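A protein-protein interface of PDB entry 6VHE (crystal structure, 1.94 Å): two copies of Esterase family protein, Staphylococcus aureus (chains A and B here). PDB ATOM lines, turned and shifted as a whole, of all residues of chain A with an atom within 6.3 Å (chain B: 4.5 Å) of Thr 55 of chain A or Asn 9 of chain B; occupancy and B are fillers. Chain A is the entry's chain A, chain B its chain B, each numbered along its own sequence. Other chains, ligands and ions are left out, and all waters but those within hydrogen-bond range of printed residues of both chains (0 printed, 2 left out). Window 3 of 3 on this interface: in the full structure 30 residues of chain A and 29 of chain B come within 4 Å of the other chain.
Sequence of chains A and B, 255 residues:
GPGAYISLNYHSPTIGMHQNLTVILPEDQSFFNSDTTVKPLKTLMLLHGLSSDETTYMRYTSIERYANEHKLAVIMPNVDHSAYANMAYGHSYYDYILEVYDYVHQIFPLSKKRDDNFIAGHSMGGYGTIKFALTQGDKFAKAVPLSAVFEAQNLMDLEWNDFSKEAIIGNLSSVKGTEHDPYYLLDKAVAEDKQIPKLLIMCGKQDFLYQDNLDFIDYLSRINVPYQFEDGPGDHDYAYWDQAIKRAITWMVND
Of the printed residues of chain B, Asp 53 of chain A touches Asn 9 (2.7 Å), His 18 (3.4 Å) and Gln 19 (3.98 Å). Of chain B, only Asn 9 comes within 4 Å of Thr 55 of chain A. Printed residues of chain B within 4 Å of Arg 59 of chain A: Asn 9 (2.8 Å) and His 18 (3.6 Å). Asn 9 of chain B touches three residues of chain A. Of the printed residues of chain A, Asn 20 of chain B touches Glu 54. The nearest residue of chain A that does not touch Asn 9 of chain B is Glu 54 of chain A (4.5 Å).
No position is printed for both chains. Of the 10 pairs that touch across the chains among the printed residues, none has its exchanged pair printed and touching as well.
Ser 52 of chain A touches His 18 of chain B (CA to ND1, 3.9 Å). Asp 53 of chain A touches His 18 of chain B. N of Gln 19 of chain B touches OD2 of Asp 53 of chain A (3.98 Å). Asn 9 of chain B touches Thr 55 of chain A. ND1 of His 18 of chain B touches CG2 of Thr 56 of chain A, at 3.5 Å. His 18 of chain B touches Arg 59 of chain A (CD2 to NH1, 3.6 Å).
The side-chain carboxylate (OD1) of Asp 53 of chain A sits at hydrogen-bond distance from the side-chain hydroxyl (OG1) of Thr 55 of chain A, at 2.8 Å. The side-chain hydroxyl (OG1) of Thr 56 of chain A sits at hydrogen-bond distance from the backbone carbonyl oxygen (O) of Asp 53 of chain A. OG1 of Thr 56 of chain A lies close to OG of Ser 52 of chain A. O of Tyr 10 of chain B lies within hydrogen-bond range of N of Gln 19 of chain B (3.1 Å). The side-chain amide nitrogen (ND2) of Asn 9 of chain B sits at hydrogen-bond distance from the side-chain amide oxygen (OD1) of Asn 20 of chain B (2.8 Å). The guanidinium group (NH1) of Arg 59 of chain A is in hydrogen-bond range of the side-chain hydroxyl (OG1) of Thr 55 of chain A (3.0 Å).
Along chain A the printed residues that touch a printed residue of chain B span positions 52 to 60. Hydrophobic or aromatic side chains of chain B that line the printed part of chain A: His 18. Among the printed residues, no Asp or Glu carboxylate lies within 4 Å of a Lys or Arg side-chain nitrogen of the other chain.
The side-chain carboxylate of Asp 53 of chain A sits at hydrogen-bond distance from the side-chain amide nitrogen of Asn 9 of chain B (2.7 Å). OD1 of Asn 9 of chain B lies within hydrogen-bond range of NH1 of Arg 59 of chain A (2.8 Å). OE2 of Glu 54 of chain A is in hydrogen-bond range of ND2 of Asn 20 of chain B (2.9 Å). The side-chain hydroxyl of Tyr 60 of chain A lies within hydrogen-bond range of a ring nitrogen (NE2) of His 18 of chain B (3.0 Å).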
ATOM      1  N   TYR A   5      -9.677  30.390  36.392  1.00  0.00           N
ATOM      2  CA  TYR A   5      -9.740  29.498  35.238  1.00  0.00           C
ATOM      3  C   TYR A   5     -10.053  30.330  34.012  1.00  0.00           C
ATOM      4  O   TYR A   5     -11.059  31.051  33.999  1.00  0.00           O
ATOM      5  CB  TYR A   5     -10.821  28.432  35.409  1.00  0.00           C
ATOM      6  CG  TYR A   5     -10.901  27.541  34.193  1.00  0.00           C
ATOM      7  CD1 TYR A   5      -9.780  26.837  33.769  1.00  0.00           C
ATOM      8  CD2 TYR A   5     -12.076  27.418  33.459  1.00  0.00           C
ATOM      9  CE1 TYR A   5      -9.822  26.025  32.664  1.00  0.00           C
ATOM     10  CE2 TYR A   5     -12.131  26.594  32.335  1.00  0.00           C
ATOM     11  CZ  TYR A   5     -10.996  25.893  31.953  1.00  0.00           C
ATOM     12  OH  TYR A   5     -11.007  25.060  30.852  1.00  0.00           O
ATOM     13  N   THR A  22      -6.443  26.996  27.207  1.00  0.00           N
ATOM     14  CA  THR A  22      -6.932  27.227  28.570  1.00  0.00           C
ATOM     15  C   THR A  22      -5.757  27.417  29.521  1.00  0.00           C
ATOM     16  O   THR A  22      -4.668  26.881  29.301  1.00  0.00           O
ATOM     17  CB  THR A  22      -7.855  26.099  29.067  1.00  0.00           C
ATOM     18  OG1 THR A  22      -7.162  24.849  29.030  1.00  0.00           O
ATOM     19  CG2 THR A  22      -9.114  26.011  28.203  1.00  0.00           C
ATOM     20  N   SER A  52      -7.856  14.233  22.675  1.00  0.00           N
ATOM     21  CA  SER A  52      -8.154  15.253  23.670  1.00  0.00           C
ATOM     22  C   SER A  52      -7.908  16.644  23.085  1.00  0.00           C
ATOM     23  O   SER A  52      -7.469  16.794  21.945  1.00  0.00           O
ATOM     24  CB  SER A  52      -7.319  15.031  24.937  1.00  0.00           C
ATOM     25  OG  SER A  52      -7.735  13.871  25.644  1.00  0.00           O
ATOM     26  N   ASP A  53      -8.182  17.681  23.871  1.00  0.00           N
ATOM     27  CA  ASP A  53      -7.964  19.059  23.411  1.00  0.00           C
ATOM     28  C   ASP A  53      -7.696  19.936  24.632  1.00  0.00           C
ATOM     29  O   ASP A  53      -7.346  19.434  25.708  1.00  0.00           O
ATOM     30  CB  ASP A  53      -9.146  19.542  22.533  1.00  0.00           C
ATOM     31  CG  ASP A  53     -10.458  19.769  23.317  1.00  0.00           C
ATOM     32  OD1 ASP A  53     -10.506  19.600  24.555  1.00  0.00           O
ATOM     33  OD2 ASP A  53     -11.473  20.122  22.671  1.00  0.00           O
ATOM     34  N   GLU A  54      -7.867  21.249  24.472  1.00  0.00           N
ATOM     35  CA  GLU A  54      -7.549  22.183  25.539  1.00  0.00           C
ATOM     36  C   GLU A  54      -8.499  22.084  26.727  1.00  0.00           C
ATOM     37  O   GLU A  54      -8.170  22.626  27.784  1.00  0.00           O
ATOM     38  CB  GLU A  54      -7.530  23.631  25.002  1.00  0.00           C
ATOM     39  CG  GLU A  54      -8.913  24.309  24.854  1.00  0.00           C
ATOM     40  CD  GLU A  54      -9.712  23.794  23.657  1.00  0.00           C
ATOM     41  OE1 GLU A  54      -9.172  22.976  22.898  1.00  0.00           O
ATOM     42  OE2 GLU A  54     -10.884  24.203  23.468  1.00  0.00           O
ATOM     43  N   THR A  55      -9.654  21.416  26.595  1.00  0.00           N
ATOM     44  CA  THR A  55     -10.628  21.363  27.682  1.00  0.00           C
ATOM     45  C   THR A  55     -10.515  20.108  28.537  1.00  0.00           C
ATOM     46  O   THR A  55     -11.055  20.084  29.646  1.00  0.00           O
ATOM     47  CB  THR A  55     -12.067  21.422  27.139  1.00  0.00           C
ATOM     48  OG1 THR A  55     -12.386  20.165  26.520  1.00  0.00           O
ATOM     49  CG2 THR A  55     -12.208  22.532  26.100  1.00  0.00           C
ATOM     50  N   THR A  56      -9.855  19.061  28.056  1.00  0.00           N
ATOM     51  CA  THR A  56     -10.148  17.764  28.648  1.00  0.00           C
ATOM     52  C   THR A  56      -9.378  17.510  29.935  1.00  0.00           C
ATOM     53  O   THR A  56      -9.821  16.689  30.732  1.00  0.00           O
ATOM     54  CB  THR A  56      -9.897  16.646  27.634  1.00  0.00           C
ATOM     55  OG1 THR A  56      -8.659  16.876  26.968  1.00  0.00           O
ATOM     56  CG2 THR A  56     -11.018  16.629  26.595  1.00  0.00           C
ATOM     57  N   TYR A  57      -8.263  18.199  30.183  1.00  0.00           N
ATOM     58  CA  TYR A  57      -7.657  18.068  31.511  1.00  0.00           C
ATOM     59  C   TYR A  57      -8.550  18.670  32.591  1.00  0.00           C
ATOM     60  O   TYR A  57      -8.709  18.083  33.670  1.00  0.00           O
ATOM     61  CB  TYR A  57      -6.260  18.695  31.542  1.00  0.00           C
ATOM     62  CG  TYR A  57      -5.167  17.641  31.535  1.00  0.00           C
ATOM     63  CD1 TYR A  57      -4.932  16.854  32.667  1.00  0.00           C
ATOM     64  CD2 TYR A  57      -4.392  17.408  30.406  1.00  0.00           C
ATOM     65  CE1 TYR A  57      -3.945  15.881  32.679  1.00  0.00           C
ATOM     66  CE2 TYR A  57      -3.396  16.416  30.407  1.00  0.00           C
ATOM     67  CZ  TYR A  57      -3.185  15.663  31.550  1.00  0.00           C
ATOM     68  OH  TYR A  57      -2.211  14.687  31.577  1.00  0.00           O
ATOM     69  N   MET A  58      -9.144  19.843  32.335  1.00  0.00           N
ATOM     70  CA  MET A  58     -10.089  20.393  33.308  1.00  0.00           C
ATOM     71  C   MET A  58     -11.247  19.435  33.535  1.00  0.00           C
ATOM     72  O   MET A  58     -11.678  19.222  34.675  1.00  0.00           O
ATOM     73  CB  MET A  58     -10.623  21.757  32.850  1.00  0.00           C
ATOM     74  CG  MET A  58     -11.731  22.338  33.775  1.00  0.00           C
ATOM     75  SD  MET A  58     -13.418  21.795  33.352  1.00  0.00           S
ATOM     76  CE  MET A  58     -13.587  22.566  31.733  1.00  0.00           C
ATOM     77  N   ARG A  59     -11.755  18.835  32.458  1.00  0.00           N
ATOM     78  CA  ARG A  59     -12.986  18.058  32.564  1.00  0.00           C
ATOM     79  C   ARG A  59     -12.783  16.721  33.280  1.00  0.00           C
ATOM     80  O   ARG A  59     -13.636  16.309  34.077  1.00  0.00           O
ATOM     81  CB  ARG A  59     -13.563  17.842  31.165  1.00  0.00           C
ATOM     82  CG  ARG A  59     -14.077  19.148  30.535  1.00  0.00           C
ATOM     83  CD  ARG A  59     -14.144  19.022  29.021  1.00  0.00           C
ATOM     84  NE  ARG A  59     -15.198  18.102  28.607  1.00  0.00           N
ATOM     85  CZ  ARG A  59     -15.560  17.919  27.346  1.00  0.00           C
ATOM     86  NH1 ARG A  59     -14.940  18.594  26.383  1.00  0.00           N
ATOM     87  NH2 ARG A  59     -16.531  17.063  27.049  1.00  0.00           N
ATOM     88  N   TYR A  60     -11.682  16.019  33.012  1.00  0.00           N
ATOM     89  CA  TYR A  60     -11.554  14.631  33.437  1.00  0.00           C
ATOM     90  C   TYR A  60     -10.599  14.429  34.607  1.00  0.00           C
ATOM     91  O   TYR A  60     -10.427  13.287  35.054  1.00  0.00           O
ATOM     92  CB  TYR A  60     -11.121  13.754  32.238  1.00  0.00           C
ATOM     93  CG  TYR A  60     -12.085  13.846  31.078  1.00  0.00           C
ATOM     94  CD1 TYR A  60     -13.461  13.863  31.295  1.00  0.00           C
ATOM     95  CD2 TYR A  60     -11.629  13.929  29.776  1.00  0.00           C
ATOM     96  CE1 TYR A  60     -14.354  13.954  30.244  1.00  0.00           C
ATOM     97  CE2 TYR A  60     -12.514  14.017  28.716  1.00  0.00           C
ATOM     98  CZ  TYR A  60     -13.870  14.035  28.955  1.00  0.00           C
ATOM     99  OH  TYR A  60     -14.743  14.129  27.898  1.00  0.00           O
ATOM    100  N   MET A  76      -2.618  24.997  28.831  1.00  0.00           N
ATOM    101  CA  MET A  76      -3.157  23.800  28.178  1.00  0.00           C
ATOM    102  C   MET A  76      -3.584  24.145  26.758  1.00  0.00           C
ATOM    103  O   MET A  76      -4.728  24.562  26.525  1.00  0.00           O
ATOM    104  CB  MET A  76      -4.324  23.211  28.973  1.00  0.00           C
ATOM    105  CG  MET A  76      -3.883  22.468  30.241  1.00  0.00           C
ATOM    106  SD  MET A  76      -5.137  22.372  31.549  1.00  0.00           S
ATOM    107  CE  MET A  76      -5.331  24.106  32.017  1.00  0.00           C
ATOM    108  N   PRO A  77      -2.689  23.977  25.778  1.00  0.00           N
ATOM    109  CA  PRO A  77      -3.054  24.279  24.389  1.00  0.00           C
ATOM    110  C   PRO A  77      -3.743  23.113  23.700  1.00  0.00           C
ATOM    111  O   PRO A  77      -3.906  22.026  24.277  1.00  0.00           O
ATOM    112  CB  PRO A  77      -1.701  24.594  23.737  1.00  0.00           C
ATOM    113  CG  PRO A  77      -0.737  23.705  24.492  1.00  0.00           C
ATOM    114  CD  PRO A  77      -1.274  23.578  25.908  1.00  0.00           C
ATOM    115  N   SER B   7     -22.025  27.036  24.160  1.00  0.00           N
ATOM    116  CA  SER B   7     -20.745  26.462  23.751  1.00  0.00           C
ATOM    117  C   SER B   7     -20.764  24.982  24.108  1.00  0.00           C
ATOM    118  O   SER B   7     -20.991  24.630  25.273  1.00  0.00           O
ATOM    119  CB  SER B   7     -19.590  27.156  24.470  1.00  0.00           C
ATOM    120  OG  SER B   7     -19.425  28.474  23.995  1.00  0.00           O
ATOM    121  N   LEU B   8     -20.533  24.123  23.118  1.00  0.00           N
ATOM    122  CA  LEU B   8     -20.515  22.679  23.320  1.00  0.00           C
ATOM    123  C   LEU B   8     -19.160  22.130  22.911  1.00  0.00           C
ATOM    124  O   LEU B   8     -18.575  22.578  21.922  1.00  0.00           O
ATOM    125  CB  LEU B   8     -21.565  21.945  22.488  1.00  0.00           C
ATOM    126  CG  LEU B   8     -23.048  22.211  22.592  1.00  0.00           C
ATOM    127  CD1 LEU B   8     -23.420  23.271  21.584  1.00  0.00           C
ATOM    128  CD2 LEU B   8     -23.786  20.900  22.331  1.00  0.00           C
ATOM    129  N   ASN B   9     -18.673  21.149  23.659  1.00  0.00           N
ATOM    130  CA  ASN B   9     -17.473  20.409  23.284  1.00  0.00           C
ATOM    131  C   ASN B   9     -17.760  18.932  23.506  1.00  0.00           C
ATOM    132  O   ASN B   9     -17.980  18.506  24.647  1.00  0.00           O
ATOM    133  CB  ASN B   9     -16.262  20.878  24.095  1.00  0.00           C
ATOM    134  CG  ASN B   9     -14.967  20.175  23.677  1.00  0.00           C
ATOM    135  OD1 ASN B   9     -14.902  18.942  23.603  1.00  0.00           O
ATOM    136  ND2 ASN B   9     -13.939  20.956  23.408  1.00  0.00           N
ATOM    137  N   TYR B  10     -17.786  18.151  22.421  1.00  0.00           N
ATOM    138  CA  TYR B  10     -17.991  16.713  22.532  1.00  0.00           C
ATOM    139  C   TYR B  10     -16.946  15.969  21.708  1.00  0.00           C
ATOM    140  O   TYR B  10     -16.371  16.512  20.759  1.00  0.00           O
ATOM    141  CB  TYR B  10     -19.426  16.304  22.117  1.00  0.00           C
ATOM    142  CG  TYR B  10     -19.748  16.335  20.634  1.00  0.00           C
ATOM    143  CD1 TYR B  10     -20.208  17.488  20.015  1.00  0.00           C
ATOM    144  CD2 TYR B  10     -19.632  15.189  19.863  1.00  0.00           C
ATOM    145  CE1 TYR B  10     -20.534  17.495  18.655  1.00  0.00           C
ATOM    146  CE2 TYR B  10     -19.955  15.191  18.517  1.00  0.00           C
ATOM    147  CZ  TYR B  10     -20.403  16.335  17.912  1.00  0.00           C
ATOM    148  OH  TYR B  10     -20.702  16.290  16.547  1.00  0.00           O
ATOM    149  N   HIS B  18     -12.170  15.443  20.603  1.00  0.00           N
ATOM    150  CA  HIS B  18     -12.986  16.528  21.134  1.00  0.00           C
ATOM    151  C   HIS B  18     -12.889  17.741  20.219  1.00  0.00           C
ATOM    152  O   HIS B  18     -11.833  18.023  19.643  1.00  0.00           O
ATOM    153  CB  HIS B  18     -12.518  16.895  22.546  1.00  0.00           C
ATOM    154  CG  HIS B  18     -12.833  15.855  23.572  1.00  0.00           C
ATOM    155  ND1 HIS B  18     -12.029  14.753  23.793  1.00  0.00           N
ATOM    156  CD2 HIS B  18     -13.863  15.752  24.448  1.00  0.00           C
ATOM    157  CE1 HIS B  18     -12.553  14.020  24.762  1.00  0.00           C
ATOM    158  NE2 HIS B  18     -13.662  14.607  25.177  1.00  0.00           N
ATOM    159  N   GLN B  19     -14.002  18.461  20.079  1.00  0.00           N
ATOM    160  CA  GLN B  19     -14.092  19.612  19.189  1.00  0.00           C
ATOM    161  C   GLN B  19     -15.163  20.552  19.736  1.00  0.00           C
ATOM    162  O   GLN B  19     -16.184  20.089  20.247  1.00  0.00           O
ATOM    163  CB  GLN B  19     -14.445  19.177  17.760  1.00  0.00           C
ATOM    164  CG  GLN B  19     -14.272  20.260  16.691  1.00  0.00           C
ATOM    165  CD  GLN B  19     -12.843  20.351  16.171  1.00  0.00           C
ATOM    166  OE1 GLN B  19     -11.886  20.008  16.873  1.00  0.00           O
ATOM    167  NE2 GLN B  19     -12.694  20.798  14.926  1.00  0.00           N
ATOM    168  N   ASN B  20     -14.922  21.861  19.639  1.00  0.00           N
ATOM    169  CA  ASN B  20     -15.879  22.864  20.105  1.00  0.00           C
ATOM    170  C   ASN B  20     -16.847  23.269  18.998  1.00  0.00           C
ATOM    171  O   ASN B  20     -16.487  23.356  17.818  1.00  0.00           O
ATOM    172  CB  ASN B  20     -15.181  24.128  20.610  1.00  0.00           C
ATOM    173  CG  ASN B  20     -14.225  23.863  21.754  1.00  0.00           C
ATOM    174  OD1 ASN B  20     -14.647  23.635  22.889  1.00  0.00           O
ATOM    175  ND2 ASN B  20     -12.918  23.913  21.462  1.00  0.00           N
